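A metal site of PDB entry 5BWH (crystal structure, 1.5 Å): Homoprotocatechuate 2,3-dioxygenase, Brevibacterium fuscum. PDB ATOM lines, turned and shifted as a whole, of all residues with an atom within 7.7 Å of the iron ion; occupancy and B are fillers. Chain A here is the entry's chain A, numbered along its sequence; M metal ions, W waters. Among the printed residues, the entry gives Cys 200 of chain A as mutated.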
ATOM      1  N   ASP A 154     -17.222  22.007   5.368  1.00  0.00           N
ATOM      2  CA  ASP A 154     -17.177  23.457   5.624  1.00  0.00           C
ATOM      3  C   ASP A 154     -18.522  24.182   5.600  1.00  0.00           C
ATOM      4  O   ASP A 154     -18.780  24.995   6.490  1.00  0.00           O
ATOM      5  CB  ASP A 154     -16.226  24.178   4.670  1.00  0.00           C
ATOM      6  CG  ASP A 154     -15.944  25.622   5.137  1.00  0.00           C
ATOM      7  OD1 ASP A 154     -15.187  25.791   6.126  1.00  0.00           O
ATOM      8  OD2 ASP A 154     -16.550  26.566   4.569  1.00  0.00           O
ATOM      9  N   HIS A 155     -19.345  23.939   4.578  1.00  0.00           N
ATOM     10  CA  HIS A 155     -20.607  24.684   4.489  1.00  0.00           C
ATOM     11  C   HIS A 155     -21.592  24.109   3.512  1.00  0.00           C
ATOM     12  O   HIS A 155     -21.268  23.237   2.699  1.00  0.00           O
ATOM     13  CB  HIS A 155     -20.355  26.187   4.164  1.00  0.00           C
ATOM     14  CG  HIS A 155     -19.776  26.448   2.808  1.00  0.00           C
ATOM     15  ND1 HIS A 155     -18.422  26.594   2.602  1.00  0.00           N
ATOM     16  CD2 HIS A 155     -20.354  26.620   1.588  1.00  0.00           C
ATOM     17  CE1 HIS A 155     -18.192  26.831   1.318  1.00  0.00           C
ATOM     18  NE2 HIS A 155     -19.344  26.875   0.693  1.00  0.00           N
ATOM     19  N   PHE A 156     -22.806  24.667   3.559  1.00  0.00           N
ATOM     20  CA  PHE A 156     -23.835  24.451   2.577  1.00  0.00           C
ATOM     21  C   PHE A 156     -24.114  25.755   1.836  1.00  0.00           C
ATOM     22  O   PHE A 156     -23.838  26.860   2.362  1.00  0.00           O
ATOM     23  CB  PHE A 156     -25.150  24.013   3.233  1.00  0.00           C
ATOM     24  CG  PHE A 156     -25.026  22.911   4.284  1.00  0.00           C
ATOM     25  CD1 PHE A 156     -24.505  21.672   3.950  1.00  0.00           C
ATOM     26  CD2 PHE A 156     -25.468  23.129   5.592  1.00  0.00           C
ATOM     27  CE1 PHE A 156     -24.433  20.665   4.904  1.00  0.00           C
ATOM     28  CE2 PHE A 156     -25.414  22.120   6.540  1.00  0.00           C
ATOM     29  CZ  PHE A 156     -24.872  20.889   6.200  1.00  0.00           C
ATOM     30  N   ASN A 157     -24.688  25.646   0.658  1.00  0.00           N
ATOM     31  CA  ASN A 157     -25.176  26.825  -0.082  1.00  0.00           C
ATOM     32  C   ASN A 157     -26.546  26.522  -0.678  1.00  0.00           C
ATOM     33  O   ASN A 157     -26.718  25.540  -1.398  1.00  0.00           O
ATOM     34  CB  ASN A 157     -24.147  27.234  -1.146  1.00  0.00           C
ATOM     35  CG  ASN A 157     -24.480  28.541  -1.818  1.00  0.00           C
ATOM     36  OD1 ASN A 157     -25.551  28.682  -2.368  1.00  0.00           O
ATOM     37  ND2 ASN A 157     -23.528  29.490  -1.820  1.00  0.00           N
ATOM     38  N   TRP A 192     -23.562  35.285   2.514  1.00  0.00           N
ATOM     39  CA  TRP A 192     -22.889  34.214   3.240  1.00  0.00           C
ATOM     40  C   TRP A 192     -22.979  34.503   4.707  1.00  0.00           C
ATOM     41  O   TRP A 192     -22.815  35.633   5.116  1.00  0.00           O
ATOM     42  CB  TRP A 192     -21.414  34.171   2.819  1.00  0.00           C
ATOM     43  CG  TRP A 192     -21.182  33.599   1.456  1.00  0.00           C
ATOM     44  CD1 TRP A 192     -20.744  32.330   1.157  1.00  0.00           C
ATOM     45  CD2 TRP A 192     -21.401  34.248   0.191  1.00  0.00           C
ATOM     46  NE1 TRP A 192     -20.652  32.165  -0.195  1.00  0.00           N
ATOM     47  CE2 TRP A 192     -21.050  33.321  -0.816  1.00  0.00           C
ATOM     48  CE3 TRP A 192     -21.827  35.528  -0.193  1.00  0.00           C
ATOM     49  CZ2 TRP A 192     -21.119  33.629  -2.178  1.00  0.00           C
ATOM     50  CZ3 TRP A 192     -21.902  35.833  -1.533  1.00  0.00           C
ATOM     51  CH2 TRP A 192     -21.558  34.893  -2.516  1.00  0.00           C
ATOM     52  N   CYS A 200     -18.590  30.959   6.049  1.00  0.00           N
ATOM     53  CA  CYS A 200     -19.943  30.522   6.210  1.00  0.00           C
ATOM     54  C   CYS A 200     -20.137  29.132   6.775  1.00  0.00           C
ATOM     55  O   CYS A 200     -19.222  28.283   6.763  1.00  0.00           O
ATOM     56  CB  CYS A 200     -20.744  30.765   4.940  1.00  0.00           C
ATOM     57  SG  CYS A 200     -20.711  29.494   3.689  1.00  0.00           S
ATOM     58  N   ALA A 203     -25.189  29.567   3.164  1.00  0.00           N
ATOM     59  CA  ALA A 203     -25.160  30.712   2.277  1.00  0.00           C
ATOM     60  C   ALA A 203     -26.421  30.681   1.459  1.00  0.00           C
ATOM     61  O   ALA A 203     -27.023  29.628   1.233  1.00  0.00           O
ATOM     62  CB  ALA A 203     -23.918  30.686   1.373  1.00  0.00           C
ATOM     63  N   THR A 205     -27.991  31.806  -2.241  1.00  0.00           N
ATOM     64  CA  THR A 205     -27.825  32.216  -3.641  1.00  0.00           C
ATOM     65  C   THR A 205     -29.191  32.523  -4.211  1.00  0.00           C
ATOM     66  O   THR A 205     -30.096  31.685  -4.129  1.00  0.00           O
ATOM     67  CB  THR A 205     -27.133  31.102  -4.438  1.00  0.00           C
ATOM     68  OG1 THR A 205     -25.852  30.825  -3.875  1.00  0.00           O
ATOM     69  CG2 THR A 205     -27.004  31.459  -5.900  1.00  0.00           C
ATOM     70  N   HIS A 213     -27.687  24.381  -3.656  1.00  0.00           N
ATOM     71  CA  HIS A 213     -26.654  24.691  -4.606  1.00  0.00           C
ATOM     72  C   HIS A 213     -25.435  23.755  -4.522  1.00  0.00           C
ATOM     73  O   HIS A 213     -25.021  23.182  -5.539  1.00  0.00           O
ATOM     74  CB  HIS A 213     -26.221  26.157  -4.506  1.00  0.00           C
ATOM     75  CG  HIS A 213     -25.503  26.609  -5.731  1.00  0.00           C
ATOM     76  ND1 HIS A 213     -24.181  26.304  -5.961  1.00  0.00           N
ATOM     77  CD2 HIS A 213     -25.943  27.251  -6.839  1.00  0.00           C
ATOM     78  CE1 HIS A 213     -23.833  26.751  -7.151  1.00  0.00           C
ATOM     79  NE2 HIS A 213     -24.875  27.337  -7.699  1.00  0.00           N
ATOM     80  N   HIS A 214     -24.856  23.658  -3.327  1.00  0.00           N
ATOM     81  CA  HIS A 214     -23.752  22.743  -3.091  1.00  0.00           C
ATOM     82  C   HIS A 214     -23.492  22.462  -1.613  1.00  0.00           C
ATOM     83  O   HIS A 214     -24.033  23.121  -0.717  1.00  0.00           O
ATOM     84  CB  HIS A 214     -22.469  23.267  -3.777  1.00  0.00           C
ATOM     85  CG  HIS A 214     -21.982  24.600  -3.287  1.00  0.00           C
ATOM     86  ND1 HIS A 214     -22.307  25.776  -3.911  1.00  0.00           N
ATOM     87  CD2 HIS A 214     -21.186  24.937  -2.241  1.00  0.00           C
ATOM     88  CE1 HIS A 214     -21.719  26.788  -3.307  1.00  0.00           C
ATOM     89  NE2 HIS A 214     -21.037  26.306  -2.278  1.00  0.00           N
ATOM     90  N   VAL A 215     -22.686  21.417  -1.396  1.00  0.00           N
ATOM     91  CA  VAL A 215     -22.059  21.123  -0.127  1.00  0.00           C
ATOM     92  C   VAL A 215     -20.569  21.298  -0.338  1.00  0.00           C
ATOM     93  O   VAL A 215     -20.050  20.850  -1.360  1.00  0.00           O
ATOM     94  CB  VAL A 215     -22.360  19.666   0.299  1.00  0.00           C
ATOM     95  CG1 VAL A 215     -21.670  19.344   1.611  1.00  0.00           C
ATOM     96  CG2 VAL A 215     -23.881  19.451   0.423  1.00  0.00           C
ATOM     97  N   ALA A 216     -19.890  21.943   0.615  1.00  0.00           N
ATOM     98  CA  ALA A 216     -18.463  22.225   0.468  1.00  0.00           C
ATOM     99  C   ALA A 216     -17.647  21.466   1.496  1.00  0.00           C
ATOM    100  O   ALA A 216     -17.953  21.519   2.697  1.00  0.00           O
ATOM    101  CB  ALA A 216     -18.198  23.720   0.619  1.00  0.00           C
ATOM    102  N   HIS A 248     -11.640  32.531  -5.026  1.00  0.00           N
ATOM    103  CA  HIS A 248     -12.855  33.312  -4.853  1.00  0.00           C
ATOM    104  C   HIS A 248     -12.504  34.750  -4.494  1.00  0.00           C
ATOM    105  O   HIS A 248     -11.522  35.016  -3.803  1.00  0.00           O
ATOM    106  CB  HIS A 248     -13.696  32.799  -3.686  1.00  0.00           C
ATOM    107  CG  HIS A 248     -14.491  31.559  -3.973  1.00  0.00           C
ATOM    108  ND1 HIS A 248     -15.358  31.451  -5.035  1.00  0.00           N
ATOM    109  CD2 HIS A 248     -14.610  30.408  -3.262  1.00  0.00           C
ATOM    110  CE1 HIS A 248     -15.964  30.281  -4.987  1.00  0.00           C
ATOM    111  NE2 HIS A 248     -15.518  29.632  -3.930  1.00  0.00           N
ATOM    112  N   SER A 251     -15.058  35.422   0.128  1.00  0.00           N
ATOM    113  CA  SER A 251     -14.443  34.378   0.991  1.00  0.00           C
ATOM    114  C   SER A 251     -12.944  34.286   0.897  1.00  0.00           C
ATOM    115  O   SER A 251     -12.317  33.807   1.838  1.00  0.00           O
ATOM    116  CB  SER A 251     -15.042  32.977   0.796  1.00  0.00           C
ATOM    117  OG  SER A 251     -14.427  32.276  -0.248  1.00  0.00           O
ATOM    118  N   TYR A 255     -10.782  27.294  -4.588  1.00  0.00           N
ATOM    119  CA  TYR A 255     -12.024  26.522  -4.786  1.00  0.00           C
ATOM    120  C   TYR A 255     -12.058  25.696  -6.068  1.00  0.00           C
ATOM    121  O   TYR A 255     -11.313  25.943  -7.023  1.00  0.00           O
ATOM    122  CB  TYR A 255     -13.270  27.445  -4.786  1.00  0.00           C
ATOM    123  CG  TYR A 255     -13.419  28.231  -6.083  1.00  0.00           C
ATOM    124  CD1 TYR A 255     -12.845  29.517  -6.228  1.00  0.00           C
ATOM    125  CD2 TYR A 255     -14.130  27.711  -7.170  1.00  0.00           C
ATOM    126  CE1 TYR A 255     -12.970  30.224  -7.412  1.00  0.00           C
ATOM    127  CE2 TYR A 255     -14.242  28.426  -8.363  1.00  0.00           C
ATOM    128  CZ  TYR A 255     -13.656  29.682  -8.470  1.00  0.00           C
ATOM    129  OH  TYR A 255     -13.788  30.376  -9.663  1.00  0.00           O
ATOM    130  N   TYR A 257     -15.488  23.361  -8.203  1.00  0.00           N
ATOM    131  CA  TYR A 257     -16.836  22.775  -8.201  1.00  0.00           C
ATOM    132  C   TYR A 257     -16.880  21.586  -9.150  1.00  0.00           C
ATOM    133  O   TYR A 257     -16.504  21.699 -10.327  1.00  0.00           O
ATOM    134  CB  TYR A 257     -17.902  23.777  -8.643  1.00  0.00           C
ATOM    135  CG  TYR A 257     -18.031  24.980  -7.751  1.00  0.00           C
ATOM    136  CD1 TYR A 257     -18.793  24.952  -6.587  1.00  0.00           C
ATOM    137  CD2 TYR A 257     -17.336  26.163  -8.040  1.00  0.00           C
ATOM    138  CE1 TYR A 257     -18.907  26.072  -5.750  1.00  0.00           C
ATOM    139  CE2 TYR A 257     -17.453  27.276  -7.224  1.00  0.00           C
ATOM    140  CZ  TYR A 257     -18.227  27.230  -6.080  1.00  0.00           C
ATOM    141  OH  TYR A 257     -18.318  28.330  -5.273  1.00  0.00           O
ATOM    142  N   GLU A 267     -18.412  21.492  -3.702  1.00  0.00           N
ATOM    143  CA  GLU A 267     -17.311  22.459  -3.712  1.00  0.00           C
ATOM    144  C   GLU A 267     -16.177  21.897  -2.871  1.00  0.00           C
ATOM    145  O   GLU A 267     -16.416  21.369  -1.792  1.00  0.00           O
ATOM    146  CB  GLU A 267     -17.748  23.806  -3.150  1.00  0.00           C
ATOM    147  CG  GLU A 267     -16.682  24.880  -3.310  1.00  0.00           C
ATOM    148  CD  GLU A 267     -17.066  26.189  -2.704  1.00  0.00           C
ATOM    149  OE1 GLU A 267     -18.093  26.256  -2.016  1.00  0.00           O
ATOM    150  OE2 GLU A 267     -16.339  27.180  -2.904  1.00  0.00           O
ATOM    151  N   ILE A 268     -14.962  22.053  -3.366  1.00  0.00           N
ATOM    152  CA  ILE A 268     -13.765  21.826  -2.595  1.00  0.00           C
ATOM    153  C   ILE A 268     -13.148  23.211  -2.355  1.00  0.00           C
ATOM    154  O   ILE A 268     -13.112  24.032  -3.262  1.00  0.00           O
ATOM    155  CB  ILE A 268     -12.766  20.902  -3.322  1.00  0.00           C
ATOM    156  CG1 ILE A 268     -13.463  19.758  -4.099  1.00  0.00           C
ATOM    157  CG2 ILE A 268     -11.777  20.360  -2.306  1.00  0.00           C
ATOM    158  CD1 ILE A 268     -14.268  18.807  -3.260  1.00  0.00           C
ATOM    159  N   TYR A 269     -12.665  23.452  -1.132  1.00  0.00           N
ATOM    160  CA  TYR A 269     -12.518  24.800  -0.581  1.00  0.00           C
ATOM    161  C   TYR A 269     -11.318  24.822   0.363  1.00  0.00           C
ATOM    162  O   TYR A 269     -11.110  23.871   1.113  1.00  0.00           O
ATOM    163  CB  TYR A 269     -13.796  25.118   0.186  1.00  0.00           C
ATOM    164  CG  TYR A 269     -14.038  26.459   0.800  1.00  0.00           C
ATOM    165  CD1 TYR A 269     -14.705  27.467   0.076  1.00  0.00           C
ATOM    166  CD2 TYR A 269     -13.750  26.698   2.131  1.00  0.00           C
ATOM    167  CE1 TYR A 269     -15.033  28.677   0.670  1.00  0.00           C
ATOM    168  CE2 TYR A 269     -14.046  27.916   2.722  1.00  0.00           C
ATOM    169  CZ  TYR A 269     -14.716  28.898   1.984  1.00  0.00           C
ATOM    170  OH  TYR A 269     -15.070  30.083   2.599  1.00  0.00           O
ATOM    171  N   ARG A 293     -16.540  36.683  -7.860  1.00  0.00           N
ATOM    172  CA  ARG A 293     -16.760  35.236  -7.743  1.00  0.00           C
ATOM    173  C   ARG A 293     -15.466  34.487  -7.976  1.00  0.00           C
ATOM    174  O   ARG A 293     -14.995  33.747  -7.125  1.00  0.00           O
ATOM    175  CB  ARG A 293     -17.916  34.752  -8.646  1.00  0.00           C
ATOM    176  CG  ARG A 293     -19.264  35.179  -8.088  1.00  0.00           C
ATOM    177  CD  ARG A 293     -20.428  34.351  -8.573  1.00  0.00           C
ATOM    178  NE  ARG A 293     -21.702  34.711  -7.931  1.00  0.00           N
ATOM    179  CZ  ARG A 293     -22.169  34.192  -6.803  1.00  0.00           C
ATOM    180  NH1 ARG A 293     -21.469  33.297  -6.117  1.00  0.00           N
ATOM    181  NH2 ARG A 293     -23.340  34.570  -6.320  1.00  0.00           N
ATOM    182  N   TRP A 304     -23.612  27.022 -13.428  1.00  0.00           N
ATOM    183  CA  TRP A 304     -23.393  27.315 -12.029  1.00  0.00           C
ATOM    184  C   TRP A 304     -24.574  28.145 -11.492  1.00  0.00           C
ATOM    185  O   TRP A 304     -24.969  28.030 -10.321  1.00  0.00           O
ATOM    186  CB  TRP A 304     -22.040  28.062 -11.838  1.00  0.00           C
ATOM    187  CG  TRP A 304     -21.562  27.992 -10.443  1.00  0.00           C
ATOM    188  CD1 TRP A 304     -20.760  27.022  -9.884  1.00  0.00           C
ATOM    189  CD2 TRP A 304     -21.863  28.913  -9.393  1.00  0.00           C
ATOM    190  NE1 TRP A 304     -20.557  27.281  -8.557  1.00  0.00           N
ATOM    191  CE2 TRP A 304     -21.208  28.438  -8.219  1.00  0.00           C
ATOM    192  CE3 TRP A 304     -22.627  30.076  -9.323  1.00  0.00           C
ATOM    193  CZ2 TRP A 304     -21.323  29.084  -7.007  1.00  0.00           C
ATOM    194  CZ3 TRP A 304     -22.724  30.724  -8.104  1.00  0.00           C
ATOM    195  CH2 TRP A 304     -22.078  30.229  -6.960  1.00  0.00           C
HETATM  196 FE    FE M   1     -19.505  27.673  -1.374  1.00  0.00          FE
HETATM  197  O   HOH W   1     -20.999  29.169  -0.475  1.00  0.00           O
HETATM  198  O   HOH W   2     -17.953  29.085  -0.993  1.00  0.00           O
HETATM  199  O   HOH W   3     -19.546  28.835  -3.209  1.00  0.00           O
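The side-chain carboxylate (OE1) of Glu 267 binds the iron ion (2.1 Å).
Water W2 is bound to the iron ion (2.1 Å).
The iron ion is bound by water W3 (2.2 Å).
NE2 of His 155 binds the iron ion (2.2 Å).
NE2 of His 214 binds the iron ion (2.2 Å).
Water W1 is bound to the iron ion, 2.3 Å away.
The iron ion has six donor atoms within binding distance.
Water W1 lies within hydrogen-bond range of the side-chain amide nitrogen (ND2) of Asn 157 and the indole nitrogen (NE1) of Trp 192.
OH of Tyr 257 lies within hydrogen-bond range of OE2 of Glu 267, at 3.3 Å.
The backbone carbonyl oxygen of His 155 is in hydrogen-bond range of the backbone NH of Ala 216 (2.8 Å).
A ring nitrogen (NE2) of His 248 sits at hydrogen-bond distance from the side-chain carboxylate (OE2) of Glu 267 (2.8 Å).
OD2 of Asp 154 is in hydrogen-bond range of ND1 of His 155, 2.7 Å away.
The backbone NH (N) of Glu 267 lies within hydrogen-bond range of the backbone carbonyl oxygen (O) of Val 215.
A ring nitrogen (ND1) of His 213 is in hydrogen-bond range of a ring nitrogen (ND1) of His 214 (2.8 Å).
The backbone carbonyl oxygen (O) of His 214 sits at hydrogen-bond distance from the backbone NH (N) of Asn 157.
The nearest printed residue that does not touch the iron ion is Tyr 257 (4.1 Å).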
